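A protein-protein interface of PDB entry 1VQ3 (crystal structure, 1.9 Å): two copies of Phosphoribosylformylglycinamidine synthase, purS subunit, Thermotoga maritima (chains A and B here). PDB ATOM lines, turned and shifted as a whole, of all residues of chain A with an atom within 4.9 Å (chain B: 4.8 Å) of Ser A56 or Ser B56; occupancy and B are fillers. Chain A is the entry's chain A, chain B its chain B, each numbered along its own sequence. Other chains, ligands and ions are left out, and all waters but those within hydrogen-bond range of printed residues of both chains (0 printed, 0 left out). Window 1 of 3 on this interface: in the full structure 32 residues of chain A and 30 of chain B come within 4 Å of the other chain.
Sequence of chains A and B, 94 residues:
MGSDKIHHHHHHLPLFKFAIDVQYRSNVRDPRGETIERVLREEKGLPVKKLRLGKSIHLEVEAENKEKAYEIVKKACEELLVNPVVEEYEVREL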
ATOM      1  N   ILE A  20      10.684  -4.924   8.225  1.00  0.00           N
ATOM      2  CA  ILE A  20       9.543  -4.901   9.176  1.00  0.00           C
ATOM      3  C   ILE A  20       8.957  -6.285   9.175  1.00  0.00           C
ATOM      4  O   ILE A  20       8.539  -6.795   8.135  1.00  0.00           O
ATOM      5  CB  ILE A  20       8.498  -3.857   8.702  1.00  0.00           C
ATOM      6  CG1 ILE A  20       9.168  -2.480   8.498  1.00  0.00           C
ATOM      7  CG2 ILE A  20       7.379  -3.693   9.732  1.00  0.00           C
ATOM      8  CD1 ILE A  20       8.380  -1.518   7.673  1.00  0.00           C
ATOM      9  N   ASP A  21       8.871  -6.878  10.348  1.00  0.00           N
ATOM     10  CA  ASP A  21       8.289  -8.182  10.548  1.00  0.00           C
ATOM     11  C   ASP A  21       6.928  -8.018  11.237  1.00  0.00           C
ATOM     12  O   ASP A  21       6.836  -7.688  12.418  1.00  0.00           O
ATOM     13  CB  ASP A  21       9.282  -8.971  11.427  1.00  0.00           C
ATOM     14  CG  ASP A  21       8.887 -10.408  11.660  1.00  0.00           C
ATOM     15  OD1 ASP A  21       7.807 -10.832  11.281  1.00  0.00           O
ATOM     16  OD2 ASP A  21       9.680 -11.209  12.167  1.00  0.00           O
ATOM     17  N   VAL A  22       5.879  -8.237  10.455  1.00  0.00           N
ATOM     18  CA  VAL A  22       4.510  -7.999  10.839  1.00  0.00           C
ATOM     19  C   VAL A  22       3.862  -9.346  11.103  1.00  0.00           C
ATOM     20  O   VAL A  22       3.856 -10.246  10.240  1.00  0.00           O
ATOM     21  CB  VAL A  22       3.684  -7.249   9.745  1.00  0.00           C
ATOM     22  CG1 VAL A  22       2.291  -6.900  10.282  1.00  0.00           C
ATOM     23  CG2 VAL A  22       4.380  -5.963   9.228  1.00  0.00           C
ATOM     24  N   GLN A  23       3.259  -9.465  12.284  1.00  0.00           N
ATOM     25  CA  GLN A  23       2.624 -10.720  12.729  1.00  0.00           C
ATOM     26  C   GLN A  23       1.289 -10.407  13.377  1.00  0.00           C
ATOM     27  O   GLN A  23       1.092  -9.315  13.938  1.00  0.00           O
ATOM     28  CB  GLN A  23       3.498 -11.439  13.779  1.00  0.00           C
ATOM     29  CG  GLN A  23       4.836 -12.029  13.264  1.00  0.00           C
ATOM     30  CD  GLN A  23       4.669 -13.141  12.231  1.00  0.00           C
ATOM     31  OE1 GLN A  23       3.686 -13.915  12.272  1.00  0.00           O
ATOM     32  NE2 GLN A  23       5.613 -13.206  11.258  1.00  0.00           N
ATOM     33  N   ARG A  52       3.906 -19.121  12.821  1.00  0.00           N
ATOM     34  CA  ARG A  52       3.156 -17.916  12.541  1.00  0.00           C
ATOM     35  C   ARG A  52       3.579 -17.316  11.243  1.00  0.00           C
ATOM     36  O   ARG A  52       4.738 -17.130  10.992  1.00  0.00           O
ATOM     37  CB  ARG A  52       3.328 -16.937  13.657  1.00  0.00           C
ATOM     38  CG  ARG A  52       2.881 -17.516  14.959  1.00  0.00           C
ATOM     39  CD  ARG A  52       2.658 -16.489  15.974  1.00  0.00           C
ATOM     40  NE  ARG A  52       3.831 -15.643  16.115  1.00  0.00           N
ATOM     41  CZ  ARG A  52       3.810 -14.379  16.521  1.00  0.00           C
ATOM     42  NH1 ARG A  52       2.658 -13.780  16.872  1.00  0.00           N
ATOM     43  NH2 ARG A  52       4.965 -13.719  16.622  1.00  0.00           N
ATOM     44  N   LEU A  53       2.598 -17.049  10.404  1.00  0.00           N
ATOM     45  CA  LEU A  53       2.814 -16.491   9.089  1.00  0.00           C
ATOM     46  C   LEU A  53       2.381 -15.021   9.144  1.00  0.00           C
ATOM     47  O   LEU A  53       1.238 -14.676   9.528  1.00  0.00           O
ATOM     48  CB  LEU A  53       2.007 -17.255   8.087  1.00  0.00           C
ATOM     49  CG  LEU A  53       1.937 -16.638   6.692  1.00  0.00           C
ATOM     50  CD1 LEU A  53       3.291 -16.673   6.057  1.00  0.00           C
ATOM     51  CD2 LEU A  53       0.839 -17.319   5.853  1.00  0.00           C
ATOM     52  N   GLY A  54       3.310 -14.160   8.781  1.00  0.00           N
ATOM     53  CA  GLY A  54       3.059 -12.731   8.700  1.00  0.00           C
ATOM     54  C   GLY A  54       3.765 -12.141   7.488  1.00  0.00           C
ATOM     55  O   GLY A  54       4.084 -12.849   6.514  1.00  0.00           O
ATOM     56  N   LYS A  55       3.978 -10.828   7.535  1.00  0.00           N
ATOM     57  CA  LYS A  55       4.510 -10.104   6.372  1.00  0.00           C
ATOM     58  C   LYS A  55       5.953  -9.747   6.696  1.00  0.00           C
ATOM     59  O   LYS A  55       6.272  -9.455   7.830  1.00  0.00           O
ATOM     60  CB  LYS A  55       3.765  -8.811   6.145  1.00  0.00           C
ATOM     61  CG  LYS A  55       2.349  -8.979   5.745  1.00  0.00           C
ATOM     62  CD  LYS A  55       1.682  -7.632   5.593  1.00  0.00           C
ATOM     63  CE  LYS A  55       0.203  -7.793   5.288  1.00  0.00           C
ATOM     64  NZ  LYS A  55      -0.512  -8.422   6.414  1.00  0.00           N
ATOM     65  N   SER A  56       6.806  -9.777   5.698  1.00  0.00           N
ATOM     66  CA  SER A  56       8.115  -9.210   5.824  1.00  0.00           C
ATOM     67  C   SER A  56       8.288  -8.095   4.816  1.00  0.00           C
ATOM     68  O   SER A  56       8.339  -8.360   3.612  1.00  0.00           O
ATOM     69  CB  SER A  56       9.187 -10.282   5.664  1.00  0.00           C
ATOM     70  OG  SER A  56      10.477  -9.650   5.628  1.00  0.00           O
ATOM     71  N   ILE A  57       8.386  -6.837   5.278  1.00  0.00           N
ATOM     72  CA  ILE A  57       8.440  -5.709   4.357  1.00  0.00           C
ATOM     73  C   ILE A  57       9.868  -5.188   4.431  1.00  0.00           C
ATOM     74  O   ILE A  57      10.359  -4.886   5.520  1.00  0.00           O
ATOM     75  CB  ILE A  57       7.375  -4.631   4.706  1.00  0.00           C
ATOM     76  CG1 ILE A  57       5.968  -5.250   4.578  1.00  0.00           C
ATOM     77  CG2 ILE A  57       7.584  -3.404   3.783  1.00  0.00           C
ATOM     78  CD1 ILE A  57       4.797  -4.462   5.193  1.00  0.00           C
ATOM     79  N   HIS A  58      10.554  -5.183   3.305  1.00  0.00           N
ATOM     80  CA  HIS A  58      11.862  -4.554   3.186  1.00  0.00           C
ATOM     81  C   HIS A  58      11.709  -3.199   2.544  1.00  0.00           C
ATOM     82  O   HIS A  58      10.940  -3.035   1.607  1.00  0.00           O
ATOM     83  CB  HIS A  58      12.882  -5.411   2.394  1.00  0.00           C
ATOM     84  CG  HIS A  58      13.277  -6.686   3.091  1.00  0.00           C
ATOM     85  ND1 HIS A  58      14.282  -7.522   2.625  1.00  0.00           N
ATOM     86  CD2 HIS A  58      12.778  -7.281   4.200  1.00  0.00           C
ATOM     87  CE1 HIS A  58      14.399  -8.553   3.445  1.00  0.00           C
ATOM     88  NE2 HIS A  58      13.486  -8.440   4.398  1.00  0.00           N
ATOM     89  N   ILE B  20      12.011 -16.895   9.457  1.00  0.00           N
ATOM     90  CA  ILE B  20      12.336 -17.003   8.044  1.00  0.00           C
ATOM     91  C   ILE B  20      11.799 -15.812   7.320  1.00  0.00           C
ATOM     92  O   ILE B  20      10.632 -15.512   7.448  1.00  0.00           O
ATOM     93  CB  ILE B  20      11.724 -18.303   7.426  1.00  0.00           C
ATOM     94  CG1 ILE B  20      12.159 -19.512   8.260  1.00  0.00           C
ATOM     95  CG2 ILE B  20      12.126 -18.398   5.989  1.00  0.00           C
ATOM     96  CD1 ILE B  20      11.282 -20.725   8.009  1.00  0.00           C
ATOM     97  N   ASP B  21      12.666 -15.146   6.554  1.00  0.00           N
ATOM     98  CA  ASP B  21      12.325 -13.987   5.725  1.00  0.00           C
ATOM     99  C   ASP B  21      12.344 -14.383   4.257  1.00  0.00           C
ATOM    100  O   ASP B  21      13.390 -14.535   3.698  1.00  0.00           O
ATOM    101  CB  ASP B  21      13.366 -12.882   5.974  1.00  0.00           C
ATOM    102  CG  ASP B  21      12.915 -11.545   5.511  1.00  0.00           C
ATOM    103  OD1 ASP B  21      12.008 -11.493   4.683  1.00  0.00           O
ATOM    104  OD2 ASP B  21      13.543 -10.494   5.832  1.00  0.00           O
ATOM    105  N   GLN B  23      11.609 -13.487   0.392  1.00  0.00           N
ATOM    106  CA  GLN B  23      11.476 -12.338  -0.493  1.00  0.00           C
ATOM    107  C   GLN B  23      11.602 -12.791  -1.951  1.00  0.00           C
ATOM    108  O   GLN B  23      12.282 -13.793  -2.264  1.00  0.00           O
ATOM    109  CB  GLN B  23      12.606 -11.326  -0.254  1.00  0.00           C
ATOM    110  CG  GLN B  23      12.603 -10.692   1.113  1.00  0.00           C
ATOM    111  CD  GLN B  23      11.416  -9.791   1.334  1.00  0.00           C
ATOM    112  OE1 GLN B  23      10.937  -9.154   0.426  1.00  0.00           O
ATOM    113  NE2 GLN B  23      10.927  -9.758   2.560  1.00  0.00           N
ATOM    114  N   ARG B  52       9.656  -3.859  -0.644  1.00  0.00           N
ATOM    115  CA  ARG B  52       9.396  -5.220  -1.116  1.00  0.00           C
ATOM    116  C   ARG B  52       8.547  -5.952  -0.113  1.00  0.00           C
ATOM    117  O   ARG B  52       8.826  -5.923   1.100  1.00  0.00           O
ATOM    118  CB  ARG B  52      10.712  -5.906  -1.462  1.00  0.00           C
ATOM    119  CG  ARG B  52      11.167  -5.344  -2.826  1.00  0.00           C
ATOM    120  CD  ARG B  52      12.359  -5.922  -3.393  1.00  0.00           C
ATOM    121  NE  ARG B  52      12.201  -7.195  -4.081  1.00  0.00           N
ATOM    122  CZ  ARG B  52      11.953  -7.362  -5.374  1.00  0.00           C
ATOM    123  NH1 ARG B  52      11.720  -6.352  -6.173  1.00  0.00           N
ATOM    124  NH2 ARG B  52      11.916  -8.577  -5.861  1.00  0.00           N
ATOM    125  N   LEU B  53       7.457  -6.544  -0.604  1.00  0.00           N
ATOM    126  CA  LEU B  53       6.576  -7.276   0.267  1.00  0.00           C
ATOM    127  C   LEU B  53       6.895  -8.748   0.151  1.00  0.00           C
ATOM    128  O   LEU B  53       6.776  -9.366  -0.909  1.00  0.00           O
ATOM    129  CB  LEU B  53       5.126  -6.947  -0.043  1.00  0.00           C
ATOM    130  CG  LEU B  53       4.086  -7.790   0.665  1.00  0.00           C
ATOM    131  CD1 LEU B  53       4.179  -7.585   2.206  1.00  0.00           C
ATOM    132  CD2 LEU B  53       2.744  -7.472   0.085  1.00  0.00           C
ATOM    133  N   GLY B  54       7.359  -9.297   1.248  1.00  0.00           N
ATOM    134  CA  GLY B  54       7.579 -10.716   1.390  1.00  0.00           C
ATOM    135  C   GLY B  54       6.870 -11.352   2.562  1.00  0.00           C
ATOM    136  O   GLY B  54       5.888 -10.824   3.096  1.00  0.00           O
ATOM    137  N   LYS B  55       7.374 -12.515   2.955  1.00  0.00           N
ATOM    138  CA  LYS B  55       6.718 -13.318   3.970  1.00  0.00           C
ATOM    139  C   LYS B  55       7.650 -13.455   5.147  1.00  0.00           C
ATOM    140  O   LYS B  55       8.866 -13.648   4.984  1.00  0.00           O
ATOM    141  CB  LYS B  55       6.316 -14.720   3.440  1.00  0.00           C
ATOM    142  CG  LYS B  55       5.232 -14.720   2.425  1.00  0.00           C
ATOM    143  CD  LYS B  55       5.473 -15.475   1.145  1.00  0.00           C
ATOM    144  CE  LYS B  55       5.962 -16.864   1.300  1.00  0.00           C
ATOM    145  NZ  LYS B  55       5.880 -17.562  -0.021  1.00  0.00           N
ATOM    146  N   SER B  56       7.060 -13.379   6.340  1.00  0.00           N
ATOM    147  CA  SER B  56       7.748 -13.736   7.559  1.00  0.00           C
ATOM    148  C   SER B  56       7.098 -14.944   8.249  1.00  0.00           C
ATOM    149  O   SER B  56       5.953 -14.892   8.686  1.00  0.00           O
ATOM    150  CB  SER B  56       7.779 -12.571   8.533  1.00  0.00           C
ATOM    151  OG  SER B  56       8.392 -12.946   9.744  1.00  0.00           O
ATOM    152  N   ILE B  57       7.888 -15.996   8.411  1.00  0.00           N
ATOM    153  CA  ILE B  57       7.418 -17.217   9.069  1.00  0.00           C
ATOM    154  C   ILE B  57       8.276 -17.417  10.328  1.00  0.00           C
ATOM    155  O   ILE B  57       9.470 -17.668  10.256  1.00  0.00           O
ATOM    156  CB  ILE B  57       7.494 -18.451   8.152  1.00  0.00           C
ATOM    157  CG1 ILE B  57       6.752 -18.237   6.836  1.00  0.00           C
ATOM    158  CG2 ILE B  57       6.962 -19.662   8.851  1.00  0.00           C
ATOM    159  CD1 ILE B  57       7.587 -17.949   5.624  1.00  0.00           C
ATOM    160  N   HIS B  58       7.633 -17.302  11.477  1.00  0.00           N
ATOM    161  CA  HIS B  58       8.233 -17.697  12.754  1.00  0.00           C
ATOM    162  C   HIS B  58       7.806 -19.140  13.032  1.00  0.00           C
ATOM    163  O   HIS B  58       6.655 -19.537  12.795  1.00  0.00           O
ATOM    164  CB  HIS B  58       7.728 -16.812  13.884  1.00  0.00           C
ATOM    165  CG  HIS B  58       8.179 -15.393  13.789  1.00  0.00           C
ATOM    166  ND1 HIS B  58       8.059 -14.515  14.834  1.00  0.00           N
ATOM    167  CD2 HIS B  58       8.685 -14.685  12.758  1.00  0.00           C
ATOM    168  CE1 HIS B  58       8.529 -13.329  14.473  1.00  0.00           C
ATOM    169  NE2 HIS B  58       8.929 -13.405  13.216  1.00  0.00           N
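Printed residues of chain B within 4 Å of Asp A21: Ser B56 and His B58. Printed residues of chain B within 4 Å of His A58: Asp B21 (2.5 Å), Gln B23 (3.4 Å) and Arg B52 (2.7 Å). Of the printed residues of chain A, Arg B52 touches Ser A56 (3.5 Å), Ile A57 (3.3 Å) and His A58 (2.7 Å). Of chain A, only Asp A21, Gln A23, Arg A52, Leu A53, Gly A54, Lys A55 and Ser A56 come within 4 Å of Ser B56. The nearest printed residue of chain A that does not touch Ser B56 is Val A22 (4.9 Å). The nearest printed residue of chain A that does not touch Ile B57 is Gln A23 (4.6 Å).
Gln A23 touches Ser B56, and with the chains exchanged Ser A56 touches Gln B23. Arg A52 touches Ser B56, and with the chains exchanged Ser A56 touches Arg B52. Gly A54 touches Lys B55, and with the chains exchanged Lys A55 touches Gly B54. Lys A55 touches Ser B56, and with the chains exchanged Ser A56 touches Lys B55.
Of the 10 printed residues of chain B, 9 touch a printed residue of chain A. Printed residues of chain A that touch a printed residue of chain B: Asp A21, Gln A23, Arg A52, Leu A53, Gly A54, Lys A55, Ser A56, Ile A57 and His A58. Hydrophobic or aromatic side chains of chain A within 4 Å of the printed part of chain B: Leu A53, Ile A57 and His A58. Among the printed residues, no Asp or Glu carboxylate lies within 4 Å of a Lys or Arg side-chain nitrogen of the other chain.
The backbone NH (N) of Ile A20 sits at hydrogen-bond distance from the backbone carbonyl oxygen (O) of Ile A57 (2.7 Å). OD1 of Asp A21 lies within hydrogen-bond range of NE2 of Gln A23 (3.2 Å). The backbone carbonyl oxygen (O) of Val A22 sits at hydrogen-bond distance from the backbone NH (N) of Lys A55 (2.8 Å). The side-chain hydroxyl (OG) of Ser A56 lies within hydrogen-bond range of a ring nitrogen (NE2) of His A58. The backbone NH of Ile B20 lies within hydrogen-bond range of the backbone carbonyl oxygen of Ile B57 (2.8 Å). The side-chain carboxylate (OD1) of Asp B21 is in hydrogen-bond range of the side-chain amide nitrogen (NE2) of Gln B23, 2.9 Å away.
Gln A23 touches His B58. Arg A52 touches Ile B57 (O to CA, 3.3 Å). Leu A53 touches Ile B57 (CD1 to CG1, 3.9 Å). O of Gly A54 touches CA of Lys B55 (3.7 Å). Gly B54 touches Lys A55. O of Arg B52 touches O of Ser A56, 3.5 Å away. Ser A56 touches Leu B53 (O to C, 3.8 Å). Ser A56 touches Lys B55. Ser A56 touches Ser B56. CD1 of Leu B53 touches CG1 of Ile A57, 3.8 Å away.
OD1 of Asp A21 is in hydrogen-bond range of OG of Ser B56. The side-chain carboxylate (OD2) of Asp A21 sits at hydrogen-bond distance from a ring nitrogen (NE2) of His B58, at 2.5 Å. NE2 of Gln A23 is in hydrogen-bond range of O of Ser B56 (3.1 Å). O of His B58 lies within hydrogen-bond range of N of Arg A52 (2.8 Å). The backbone NH (N) of Gly A54 sits at hydrogen-bond distance from the backbone carbonyl oxygen (O) of Ser B56 (2.7 Å). The side-chain carboxylate (OD1) of Asp B21 sits at hydrogen-bond distance from the side-chain hydroxyl (OG) of Ser A56 (2.6 Å). OG of Ser A56 lies within hydrogen-bond range of NE2 of Gln B23, at 3.1 Å. The backbone NH of Gly B54 is in hydrogen-bond range of the backbone carbonyl oxygen of Ser A56 (2.7 Å). A ring nitrogen (NE2) of His A58 sits at hydrogen-bond distance from the side-chain carboxylate of Asp B21, 2.5 Å away. A ring nitrogen (NE2) of His A58 lies within hydrogen-bond range of the side-chain amide nitrogen (NE2) of Gln B23. The backbone NH (N) of Arg B52 lies within hydrogen-bond range of the backbone carbonyl oxygen (O) of His A58. The backbone carbonyl oxygen (O) of Ser B56 lies close to the backbone carbonyl oxygen (O) of Arg A52 (3.4 Å).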
